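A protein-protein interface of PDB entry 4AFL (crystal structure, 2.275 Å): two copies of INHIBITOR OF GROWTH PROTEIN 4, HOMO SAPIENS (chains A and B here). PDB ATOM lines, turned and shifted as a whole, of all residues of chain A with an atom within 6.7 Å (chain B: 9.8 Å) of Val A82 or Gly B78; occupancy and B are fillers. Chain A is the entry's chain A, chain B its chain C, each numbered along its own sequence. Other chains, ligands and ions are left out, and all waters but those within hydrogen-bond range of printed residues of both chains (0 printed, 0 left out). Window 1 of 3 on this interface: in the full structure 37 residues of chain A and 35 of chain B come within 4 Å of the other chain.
NZ of Lys B75 lies within salt-bridge range of OD2 of Asp B79 (2.7 Å).
Met A27 touches Lys B38 (CG to CE, 3.6 Å). Gly A78 touches Val B82. Val B82 touches Asp A79. CD of Lys B75 touches CG1 of Val A82 (3.9 Å). C of Gly B78 touches CG2 of Val A82 (3.5 Å). CG1 of Val A82 touches OD1 of Asp B79, 3.5 Å away. Ala A85 touches Lys B75.
Gln A83 touches none of the printed residues of chain B. Of the printed residues of chain A, Asp B79 touches Val A82 (3.5 Å). Of the printed residues of chain B, Gly A78 touches Val B82. The nearest residue of chain A that does not touch Gly B78 is Gly A78 (5.0 Å).
Of the 13 printed residues of chain A, 5 touch a printed residue of chain B. Of the 25 printed residues of chain B, 5 touch a printed residue of chain A. Along chain B the printed residues that touch a printed residue of chain A span positions 38 to 82. Among the printed residues, 7 pairs touch across the chains. Among the printed residues, no Asp or Glu carboxylate lies within 4 Å of a Lys or Arg side-chain nitrogen of the other chain.
Gly A78 touches Val B82, and with the chains exchanged Val A82 touches Gly B78. Asp A79 touches Val B82, and with the chains exchanged Val A82 touches Asp B79. Of the 7 pairs that touch across the chains among the printed residues, 4 have their exchanged pair printed and touching as well.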
ATOM      1  N   MET A  27       2.596 -19.507   2.261  1.00  0.00           N
ATOM      2  CA  MET A  27       3.441 -18.606   1.487  1.00  0.00           C
ATOM      3  C   MET A  27       2.611 -17.776   0.523  1.00  0.00           C
ATOM      4  O   MET A  27       2.713 -16.551   0.494  1.00  0.00           O
ATOM      5  CB  MET A  27       4.457 -19.412   0.685  1.00  0.00           C
ATOM      6  CG  MET A  27       5.472 -18.540  -0.024  1.00  0.00           C
ATOM      7  SD  MET A  27       6.530 -17.487   1.269  1.00  0.00           S
ATOM      8  CE  MET A  27       7.955 -18.805   1.593  1.00  0.00           C
ATOM      9  N   LEU A  30       0.877 -15.135   2.362  1.00  0.00           N
ATOM     10  CA  LEU A  30       1.725 -14.022   2.757  1.00  0.00           C
ATOM     11  C   LEU A  30       2.091 -13.217   1.520  1.00  0.00           C
ATOM     12  O   LEU A  30       2.313 -12.010   1.596  1.00  0.00           O
ATOM     13  CB  LEU A  30       2.996 -14.522   3.440  1.00  0.00           C
ATOM     14  CG  LEU A  30       2.784 -15.210   4.781  1.00  0.00           C
ATOM     15  CD1 LEU A  30       3.974 -16.087   5.099  1.00  0.00           C
ATOM     16  CD2 LEU A  30       2.575 -14.166   5.864  1.00  0.00           C
ATOM     17  N   PHE A  77       6.092  -8.909   7.068  1.00  0.00           N
ATOM     18  CA  PHE A  77       5.636 -10.028   6.269  1.00  0.00           C
ATOM     19  C   PHE A  77       6.830 -10.757   5.669  1.00  0.00           C
ATOM     20  O   PHE A  77       6.842 -11.984   5.585  1.00  0.00           O
ATOM     21  CB  PHE A  77       4.644  -9.562   5.211  1.00  0.00           C
ATOM     22  CG  PHE A  77       3.258  -9.310   5.762  1.00  0.00           C
ATOM     23  CD1 PHE A  77       2.702 -10.190   6.679  1.00  0.00           C
ATOM     24  CD2 PHE A  77       2.528  -8.189   5.380  1.00  0.00           C
ATOM     25  CE1 PHE A  77       1.440  -9.968   7.198  1.00  0.00           C
ATOM     26  CE2 PHE A  77       1.258  -7.961   5.887  1.00  0.00           C
ATOM     27  CZ  PHE A  77       0.711  -8.850   6.804  1.00  0.00           C
ATOM     28  N   GLY A  78       7.842  -9.993   5.274  1.00  0.00           N
ATOM     29  CA  GLY A  78       9.105 -10.568   4.871  1.00  0.00           C
ATOM     30  C   GLY A  78       9.699 -11.442   5.963  1.00  0.00           C
ATOM     31  O   GLY A  78      10.193 -12.526   5.689  1.00  0.00           O
ATOM     32  N   ASP A  79       9.655 -10.972   7.205  1.00  0.00           N
ATOM     33  CA  ASP A  79      10.134 -11.768   8.336  1.00  0.00           C
ATOM     34  C   ASP A  79       9.423 -13.113   8.362  1.00  0.00           C
ATOM     35  O   ASP A  79      10.056 -14.161   8.493  1.00  0.00           O
ATOM     36  CB  ASP A  79       9.888 -11.036   9.656  1.00  0.00           C
ATOM     37  CG  ASP A  79      10.886  -9.918   9.901  1.00  0.00           C
ATOM     38  OD1 ASP A  79      12.055 -10.072   9.495  1.00  0.00           O
ATOM     39  OD2 ASP A  79      10.504  -8.890  10.507  1.00  0.00           O
ATOM     40  N   ASP A  80       8.099 -13.067   8.218  1.00  0.00           N
ATOM     41  CA  ASP A  80       7.273 -14.261   8.167  1.00  0.00           C
ATOM     42  C   ASP A  80       7.575 -15.189   6.985  1.00  0.00           C
ATOM     43  O   ASP A  80       7.485 -16.409   7.133  1.00  0.00           O
ATOM     44  CB  ASP A  80       5.796 -13.890   8.159  1.00  0.00           C
ATOM     45  CG  ASP A  80       5.397 -13.048   9.360  1.00  0.00           C
ATOM     46  OD1 ASP A  80       6.191 -12.966  10.327  1.00  0.00           O
ATOM     47  OD2 ASP A  80       4.280 -12.477   9.338  1.00  0.00           O
ATOM     48  N   LYS A  81       7.914 -14.633   5.819  1.00  0.00           N
ATOM     49  CA  LYS A  81       8.189 -15.481   4.659  1.00  0.00           C
ATOM     50  C   LYS A  81       9.546 -16.145   4.806  1.00  0.00           C
ATOM     51  O   LYS A  81       9.744 -17.290   4.411  1.00  0.00           O
ATOM     52  CB  LYS A  81       8.182 -14.681   3.368  1.00  0.00           C
ATOM     53  CG  LYS A  81       6.820 -14.302   2.860  1.00  0.00           C
ATOM     54  CD  LYS A  81       7.006 -13.550   1.553  1.00  0.00           C
ATOM     55  CE  LYS A  81       5.801 -12.692   1.207  1.00  0.00           C
ATOM     56  NZ  LYS A  81       6.071 -11.881  -0.019  1.00  0.00           N
ATOM     57  N   VAL A  82      10.484 -15.394   5.365  1.00  0.00           N
ATOM     58  CA  VAL A  82      11.818 -15.898   5.614  1.00  0.00           C
ATOM     59  C   VAL A  82      11.786 -17.052   6.608  1.00  0.00           C
ATOM     60  O   VAL A  82      12.382 -18.104   6.347  1.00  0.00           O
ATOM     61  CB  VAL A  82      12.743 -14.781   6.097  1.00  0.00           C
ATOM     62  CG1 VAL A  82      14.049 -15.354   6.619  1.00  0.00           C
ATOM     63  CG2 VAL A  82      12.990 -13.823   4.964  1.00  0.00           C
ATOM     64  N   GLN A  83      11.069 -16.870   7.723  1.00  0.00           N
ATOM     65  CA  GLN A  83      10.897 -17.950   8.696  1.00  0.00           C
ATOM     66  C   GLN A  83      10.323 -19.200   8.030  1.00  0.00           C
ATOM     67  O   GLN A  83      10.883 -20.291   8.142  1.00  0.00           O
ATOM     68  CB  GLN A  83       9.990 -17.526   9.844  1.00  0.00           C
ATOM     69  CG  GLN A  83      10.719 -16.824  10.969  1.00  0.00           C
ATOM     70  CD  GLN A  83      11.926 -17.604  11.469  1.00  0.00           C
ATOM     71  OE1 GLN A  83      11.858 -18.818  11.684  1.00  0.00           O
ATOM     72  NE2 GLN A  83      13.043 -16.904  11.649  1.00  0.00           N
ATOM     73  N   LEU A  84       9.209 -19.020   7.330  1.00  0.00           N
ATOM     74  CA  LEU A  84       8.532 -20.118   6.660  1.00  0.00           C
ATOM     75  C   LEU A  84       9.465 -20.795   5.661  1.00  0.00           C
ATOM     76  O   LEU A  84       9.549 -22.021   5.615  1.00  0.00           O
ATOM     77  CB  LEU A  84       7.260 -19.610   5.977  1.00  0.00           C
ATOM     78  CG  LEU A  84       6.414 -20.605   5.185  1.00  0.00           C
ATOM     79  CD1 LEU A  84       5.813 -21.682   6.090  1.00  0.00           C
ATOM     80  CD2 LEU A  84       5.328 -19.868   4.389  1.00  0.00           C
ATOM     81  N   ALA A  85      10.197 -19.997   4.893  1.00  0.00           N
ATOM     82  CA  ALA A  85      11.156 -20.551   3.952  1.00  0.00           C
ATOM     83  C   ALA A  85      12.210 -21.364   4.682  1.00  0.00           C
ATOM     84  O   ALA A  85      12.533 -22.466   4.264  1.00  0.00           O
ATOM     85  CB  ALA A  85      11.807 -19.450   3.126  1.00  0.00           C
ATOM     86  N   MET A  86      12.748 -20.827   5.772  1.00  0.00           N
ATOM     87  CA  MET A  86      13.713 -21.570   6.576  1.00  0.00           C
ATOM     88  C   MET A  86      13.136 -22.897   7.009  1.00  0.00           C
ATOM     89  O   MET A  86      13.781 -23.931   6.864  1.00  0.00           O
ATOM     90  CB  MET A  86      14.106 -20.799   7.825  1.00  0.00           C
ATOM     91  CG  MET A  86      14.982 -19.613   7.555  1.00  0.00           C
ATOM     92  SD  MET A  86      15.465 -18.735   9.215  1.00  0.00           S
ATOM     93  CE  MET A  86      16.466 -20.242  10.045  1.00  0.00           C
ATOM     94  N   GLN A  87      11.917 -22.865   7.536  1.00  0.00           N
ATOM     95  CA  GLN A  87      11.296 -24.076   8.058  1.00  0.00           C
ATOM     96  C   GLN A  87      11.075 -25.116   6.959  1.00  0.00           C
ATOM     97  O   GLN A  87      11.294 -26.308   7.177  1.00  0.00           O
ATOM     98  CB  GLN A  87       9.983 -23.757   8.777  1.00  0.00           C
ATOM     99  CG  GLN A  87      10.159 -22.828   9.957  1.00  0.00           C
ATOM    100  CD  GLN A  87       8.840 -22.325  10.522  1.00  0.00           C
ATOM    101  OE1 GLN A  87       7.762 -22.739  10.085  1.00  0.00           O
ATOM    102  NE2 GLN A  87       8.920 -21.422  11.501  1.00  0.00           N
ATOM    103  N   MET B  27      13.021  -3.820  -5.232  1.00  0.00           N
ATOM    104  CA  MET B  27      12.009  -4.685  -4.659  1.00  0.00           C
ATOM    105  C   MET B  27      11.248  -5.472  -5.736  1.00  0.00           C
ATOM    106  O   MET B  27      10.925  -6.637  -5.558  1.00  0.00           O
ATOM    107  CB  MET B  27      11.024  -3.879  -3.844  1.00  0.00           C
ATOM    108  CG  MET B  27      10.006  -4.750  -3.202  1.00  0.00           C
ATOM    109  SD  MET B  27      10.864  -5.753  -1.740  1.00  0.00           S
ATOM    110  CE  MET B  27      10.973  -4.281  -0.426  1.00  0.00           C
ATOM    111  N   LEU B  30      13.510  -8.336  -7.029  1.00  0.00           N
ATOM    112  CA  LEU B  30      13.528  -9.405  -6.042  1.00  0.00           C
ATOM    113  C   LEU B  30      12.229 -10.211  -6.068  1.00  0.00           C
ATOM    114  O   LEU B  30      12.255 -11.435  -5.903  1.00  0.00           O
ATOM    115  CB  LEU B  30      13.759  -8.822  -4.654  1.00  0.00           C
ATOM    116  CG  LEU B  30      15.155  -8.254  -4.428  1.00  0.00           C
ATOM    117  CD1 LEU B  30      15.134  -7.191  -3.342  1.00  0.00           C
ATOM    118  CD2 LEU B  30      16.117  -9.377  -4.047  1.00  0.00           C
ATOM    119  N   ASP B  31      11.100  -9.532  -6.278  1.00  0.00           N
ATOM    120  CA  ASP B  31       9.811 -10.226  -6.345  1.00  0.00           C
ATOM    121  C   ASP B  31       9.730 -11.095  -7.588  1.00  0.00           C
ATOM    122  O   ASP B  31       9.144 -12.179  -7.563  1.00  0.00           O
ATOM    123  CB  ASP B  31       8.637  -9.248  -6.326  1.00  0.00           C
ATOM    124  CG  ASP B  31       8.443  -8.599  -4.968  1.00  0.00           C
ATOM    125  OD1 ASP B  31       8.789  -9.233  -3.952  1.00  0.00           O
ATOM    126  OD2 ASP B  31       7.937  -7.454  -4.915  1.00  0.00           O
ATOM    127  N   ARG B  33      12.242 -12.536  -8.927  1.00  0.00           N
ATOM    128  CA  ARG B  33      13.070 -13.697  -8.644  1.00  0.00           C
ATOM    129  C   ARG B  33      12.323 -14.725  -7.801  1.00  0.00           C
ATOM    130  O   ARG B  33      12.298 -15.905  -8.153  1.00  0.00           O
ATOM    131  CB  ARG B  33      14.387 -13.286  -8.003  1.00  0.00           C
ATOM    132  CG  ARG B  33      15.375 -12.733  -9.024  1.00  0.00           C
ATOM    133  CD  ARG B  33      16.591 -12.153  -8.343  1.00  0.00           C
ATOM    134  NE  ARG B  33      17.750 -12.078  -9.232  1.00  0.00           N
ATOM    135  CZ  ARG B  33      17.967 -11.098 -10.106  1.00  0.00           C
ATOM    136  NH1 ARG B  33      17.099 -10.101 -10.226  1.00  0.00           N
ATOM    137  NH2 ARG B  33      19.053 -11.117 -10.867  1.00  0.00           N
ATOM    138  N   THR B  34      11.670 -14.286  -6.726  1.00  0.00           N
ATOM    139  CA  THR B  34      10.949 -15.249  -5.901  1.00  0.00           C
ATOM    140  C   THR B  34       9.712 -15.840  -6.586  1.00  0.00           C
ATOM    141  O   THR B  34       9.458 -17.037  -6.441  1.00  0.00           O
ATOM    142  CB  THR B  34      10.627 -14.725  -4.485  1.00  0.00           C
ATOM    143  OG1 THR B  34       9.608 -13.716  -4.548  1.00  0.00           O
ATOM    144  CG2 THR B  34      11.883 -14.166  -3.847  1.00  0.00           C
ATOM    145  N   GLU B  35       8.970 -15.034  -7.348  1.00  0.00           N
ATOM    146  CA  GLU B  35       7.849 -15.582  -8.123  1.00  0.00           C
ATOM    147  C   GLU B  35       8.339 -16.720  -9.009  1.00  0.00           C
ATOM    148  O   GLU B  35       7.767 -17.803  -9.008  1.00  0.00           O
ATOM    149  CB  GLU B  35       7.150 -14.504  -8.970  1.00  0.00           C
ATOM    150  N   LEU B  37      10.974 -18.563  -8.677  1.00  0.00           N
ATOM    151  CA  LEU B  37      11.409 -19.694  -7.896  1.00  0.00           C
ATOM    152  C   LEU B  37      10.205 -20.479  -7.394  1.00  0.00           C
ATOM    153  O   LEU B  37      10.200 -21.704  -7.424  1.00  0.00           O
ATOM    154  CB  LEU B  37      12.269 -19.229  -6.735  1.00  0.00           C
ATOM    155  CG  LEU B  37      13.719 -18.883  -7.054  1.00  0.00           C
ATOM    156  CD1 LEU B  37      14.396 -18.375  -5.799  1.00  0.00           C
ATOM    157  CD2 LEU B  37      14.454 -20.102  -7.606  1.00  0.00           C
ATOM    158  N   LYS B  38       9.176 -19.767  -6.950  1.00  0.00           N
ATOM    159  CA  LYS B  38       7.997 -20.426  -6.418  1.00  0.00           C
ATOM    160  C   LYS B  38       7.313 -21.236  -7.505  1.00  0.00           C
ATOM    161  O   LYS B  38       6.808 -22.315  -7.241  1.00  0.00           O
ATOM    162  CB  LYS B  38       7.052 -19.420  -5.761  1.00  0.00           C
ATOM    163  CG  LYS B  38       7.584 -18.952  -4.409  1.00  0.00           C
ATOM    164  CD  LYS B  38       7.061 -17.571  -3.998  1.00  0.00           C
ATOM    165  CE  LYS B  38       7.609 -17.178  -2.621  1.00  0.00           C
ATOM    166  NZ  LYS B  38       7.248 -15.789  -2.202  1.00  0.00           N
ATOM    167  N   ALA B  70      16.060 -24.440  -4.358  1.00  0.00           N
ATOM    168  CA  ALA B  70      15.116 -23.384  -4.693  1.00  0.00           C
ATOM    169  C   ALA B  70      14.599 -22.665  -3.443  1.00  0.00           C
ATOM    170  O   ALA B  70      14.456 -21.451  -3.434  1.00  0.00           O
ATOM    171  CB  ALA B  70      13.967 -23.939  -5.503  1.00  0.00           C
ATOM    172  N   TYR B  71      14.330 -23.408  -2.379  1.00  0.00           N
ATOM    173  CA  TYR B  71      13.878 -22.753  -1.162  1.00  0.00           C
ATOM    174  C   TYR B  71      14.991 -21.947  -0.497  1.00  0.00           C
ATOM    175  O   TYR B  71      14.758 -20.856   0.014  1.00  0.00           O
ATOM    176  CB  TYR B  71      13.274 -23.758  -0.201  1.00  0.00           C
ATOM    177  CG  TYR B  71      11.774 -23.837  -0.302  1.00  0.00           C
ATOM    178  CD1 TYR B  71      10.972 -22.781   0.138  1.00  0.00           C
ATOM    179  CD2 TYR B  71      11.150 -24.959  -0.821  1.00  0.00           C
ATOM    180  CE1 TYR B  71       9.591 -22.850   0.056  1.00  0.00           C
ATOM    181  CE2 TYR B  71       9.768 -25.038  -0.904  1.00  0.00           C
ATOM    182  CZ  TYR B  71       8.996 -23.983  -0.463  1.00  0.00           C
ATOM    183  OH  TYR B  71       7.621 -24.061  -0.551  1.00  0.00           O
ATOM    184  N   GLY B  72      16.203 -22.486  -0.512  1.00  0.00           N
ATOM    185  CA  GLY B  72      17.360 -21.775  -0.005  1.00  0.00           C
ATOM    186  C   GLY B  72      17.532 -20.430  -0.691  1.00  0.00           C
ATOM    187  O   GLY B  72      17.812 -19.436  -0.031  1.00  0.00           O
ATOM    188  N   LYS B  73      17.371 -20.402  -2.011  1.00  0.00           N
ATOM    189  CA  LYS B  73      17.522 -19.166  -2.782  1.00  0.00           C
ATOM    190  C   LYS B  73      16.398 -18.193  -2.434  1.00  0.00           C
ATOM    191  O   LYS B  73      16.604 -16.987  -2.317  1.00  0.00           O
ATOM    192  CB  LYS B  73      17.490 -19.458  -4.283  1.00  0.00           C
ATOM    193  CG  LYS B  73      18.694 -20.224  -4.828  1.00  0.00           C
ATOM    194  CD  LYS B  73      18.575 -20.382  -6.347  1.00  0.00           C
ATOM    195  CE  LYS B  73      19.866 -20.895  -6.985  1.00  0.00           C
ATOM    196  NZ  LYS B  73      19.942 -22.387  -7.068  1.00  0.00           N
ATOM    197  N   CYS B  74      15.203 -18.745  -2.275  1.00  0.00           N
ATOM    198  CA  CYS B  74      14.024 -17.981  -1.892  1.00  0.00           C
ATOM    199  C   CYS B  74      14.215 -17.303  -0.532  1.00  0.00           C
ATOM    200  O   CYS B  74      13.977 -16.107  -0.396  1.00  0.00           O
ATOM    201  CB  CYS B  74      12.814 -18.912  -1.848  1.00  0.00           C
ATOM    202  SG  CYS B  74      11.258 -18.165  -2.260  1.00  0.00           S
ATOM    203  N   LYS B  75      14.647 -18.062   0.475  1.00  0.00           N
ATOM    204  CA  LYS B  75      14.887 -17.476   1.782  1.00  0.00           C
ATOM    205  C   LYS B  75      15.918 -16.344   1.682  1.00  0.00           C
ATOM    206  O   LYS B  75      15.717 -15.274   2.264  1.00  0.00           O
ATOM    207  CB  LYS B  75      15.209 -18.546   2.845  1.00  0.00           C
ATOM    208  CG  LYS B  75      16.575 -18.474   3.522  1.00  0.00           C
ATOM    209  CD  LYS B  75      16.672 -17.425   4.628  1.00  0.00           C
ATOM    210  CE  LYS B  75      18.039 -17.548   5.310  1.00  0.00           C
ATOM    211  NZ  LYS B  75      18.391 -16.430   6.217  1.00  0.00           N
ATOM    212  N   GLU B  76      16.985 -16.540   0.908  1.00  0.00           N
ATOM    213  CA  GLU B  76      17.987 -15.478   0.784  1.00  0.00           C
ATOM    214  C   GLU B  76      17.506 -14.245   0.023  1.00  0.00           C
ATOM    215  O   GLU B  76      17.879 -13.114   0.361  1.00  0.00           O
ATOM    216  CB  GLU B  76      19.309 -16.013   0.257  1.00  0.00           C
ATOM    217  CG  GLU B  76      20.080 -16.694   1.378  1.00  0.00           C
ATOM    218  CD  GLU B  76      21.346 -17.353   0.909  1.00  0.00           C
ATOM    219  OE1 GLU B  76      21.728 -17.127  -0.258  1.00  0.00           O
ATOM    220  OE2 GLU B  76      21.955 -18.100   1.711  1.00  0.00           O
ATOM    221  N   PHE B  77      16.666 -14.458  -0.986  1.00  0.00           N
ATOM    222  CA  PHE B  77      16.006 -13.336  -1.622  1.00  0.00           C
ATOM    223  C   PHE B  77      15.054 -12.710  -0.618  1.00  0.00           C
ATOM    224  O   PHE B  77      14.857 -11.503  -0.610  1.00  0.00           O
ATOM    225  CB  PHE B  77      15.305 -13.750  -2.923  1.00  0.00           C
ATOM    226  CG  PHE B  77      16.258 -13.956  -4.085  1.00  0.00           C
ATOM    227  CD1 PHE B  77      17.318 -13.082  -4.293  1.00  0.00           C
ATOM    228  CD2 PHE B  77      16.115 -15.032  -4.938  1.00  0.00           C
ATOM    229  CE1 PHE B  77      18.204 -13.265  -5.348  1.00  0.00           C
ATOM    230  CE2 PHE B  77      16.990 -15.220  -5.999  1.00  0.00           C
ATOM    231  CZ  PHE B  77      18.042 -14.341  -6.199  1.00  0.00           C
ATOM    232  N   GLY B  78      14.491 -13.532   0.260  1.00  0.00           N
ATOM    233  CA  GLY B  78      13.649 -13.027   1.326  1.00  0.00           C
ATOM    234  C   GLY B  78      14.421 -12.126   2.282  1.00  0.00           C
ATOM    235  O   GLY B  78      13.899 -11.092   2.696  1.00  0.00           O
ATOM    236  N   ASP B  79      15.644 -12.519   2.657  1.00  0.00           N
ATOM    237  CA  ASP B  79      16.492 -11.665   3.498  1.00  0.00           C
ATOM    238  C   ASP B  79      16.737 -10.331   2.785  1.00  0.00           C
ATOM    239  O   ASP B  79      16.718  -9.266   3.403  1.00  0.00           O
ATOM    240  CB  ASP B  79      17.841 -12.315   3.812  1.00  0.00           C
ATOM    241  CG  ASP B  79      17.715 -13.604   4.619  1.00  0.00           C
ATOM    242  OD1 ASP B  79      16.908 -13.645   5.569  1.00  0.00           O
ATOM    243  OD2 ASP B  79      18.444 -14.579   4.307  1.00  0.00           O
ATOM    244  N   ASP B  80      16.963 -10.399   1.481  1.00  0.00           N
ATOM    245  CA  ASP B  80      17.220  -9.194   0.700  1.00  0.00           C
ATOM    246  C   ASP B  80      16.048  -8.219   0.757  1.00  0.00           C
ATOM    247  O   ASP B  80      16.246  -7.029   0.973  1.00  0.00           O
ATOM    248  CB  ASP B  80      17.550  -9.547  -0.747  1.00  0.00           C
ATOM    249  CG  ASP B  80      18.860 -10.296  -0.873  1.00  0.00           C
ATOM    250  OD1 ASP B  80      19.718 -10.136   0.025  1.00  0.00           O
ATOM    251  OD2 ASP B  80      19.039 -11.035  -1.862  1.00  0.00           O
ATOM    252  N   LYS B  81      14.835  -8.726   0.586  1.00  0.00           N
ATOM    253  CA  LYS B  81      13.656  -7.876   0.655  1.00  0.00           C
ATOM    254  C   LYS B  81      13.505  -7.271   2.038  1.00  0.00           C
ATOM    255  O   LYS B  81      13.170  -6.102   2.168  1.00  0.00           O
ATOM    256  CB  LYS B  81      12.389  -8.653   0.313  1.00  0.00           C
ATOM    257  CG  LYS B  81      12.289  -9.115  -1.117  1.00  0.00           C
ATOM    258  CD  LYS B  81      11.112 -10.066  -1.195  1.00  0.00           C
ATOM    259  CE  LYS B  81      11.073 -10.835  -2.487  1.00  0.00           C
ATOM    260  NZ  LYS B  81       9.980 -11.838  -2.402  1.00  0.00           N
ATOM    261  N   VAL B  82      13.748  -8.076   3.067  1.00  0.00           N
ATOM    262  CA  VAL B  82      13.666  -7.603   4.437  1.00  0.00           C
ATOM    263  C   VAL B  82      14.662  -6.475   4.693  1.00  0.00           C
ATOM    264  O   VAL B  82      14.273  -5.405   5.162  1.00  0.00           O
ATOM    265  CB  VAL B  82      13.882  -8.753   5.452  1.00  0.00           C
ATOM    266  CG1 VAL B  82      14.137  -8.191   6.847  1.00  0.00           C
ATOM    267  CG2 VAL B  82      12.681  -9.671   5.466  1.00  0.00           C
ATOM    268  N   GLN B  83      15.939  -6.720   4.393  1.00  0.00           N
ATOM    269  CA  GLN B  83      16.967  -5.680   4.472  1.00  0.00           C
ATOM    270  C   GLN B  83      16.607  -4.438   3.636  1.00  0.00           C
ATOM    271  O   GLN B  83      16.849  -3.306   4.037  1.00  0.00           O
ATOM    272  CB  GLN B  83      18.327  -6.237   4.053  1.00  0.00           C
ATOM    273  N   LEU B  84      16.019  -4.649   2.469  1.00  0.00           N
ATOM    274  CA  LEU B  84      15.646  -3.515   1.638  1.00  0.00           C
ATOM    275  C   LEU B  84      14.478  -2.699   2.258  1.00  0.00           C
ATOM    276  O   LEU B  84      14.501  -1.460   2.251  1.00  0.00           O
ATOM    277  CB  LEU B  84      15.306  -4.000   0.239  1.00  0.00           C
ATOM    278  CG  LEU B  84      14.833  -2.994  -0.802  1.00  0.00           C
ATOM    279  CD1 LEU B  84      15.793  -1.805  -0.893  1.00  0.00           C
ATOM    280  CD2 LEU B  84      14.696  -3.713  -2.148  1.00  0.00           C
ATOM    281  N   ALA B  85      13.480  -3.393   2.801  1.00  0.00           N
ATOM    282  CA  ALA B  85      12.341  -2.740   3.435  1.00  0.00           C
ATOM    283  C   ALA B  85      12.792  -1.983   4.670  1.00  0.00           C
ATOM    284  O   ALA B  85      12.330  -0.881   4.922  1.00  0.00           O
ATOM    285  CB  ALA B  85      11.274  -3.771   3.820  1.00  0.00           C
ATOM    286  N   MET B  86      13.693  -2.582   5.443  1.00  0.00           N
ATOM    287  CA  MET B  86      14.217  -1.914   6.626  1.00  0.00           C
ATOM    288  C   MET B  86      15.021  -0.680   6.266  1.00  0.00           C
ATOM    289  O   MET B  86      14.915   0.339   6.940  1.00  0.00           O
ATOM    290  CB  MET B  86      15.129  -2.829   7.428  1.00  0.00           C
ATOM    291  CG  MET B  86      14.425  -3.896   8.197  1.00  0.00           C
ATOM    292  SD  MET B  86      15.745  -4.994   9.141  1.00  0.00           S
ATOM    293  CE  MET B  86      16.609  -3.568  10.160  1.00  0.00           C
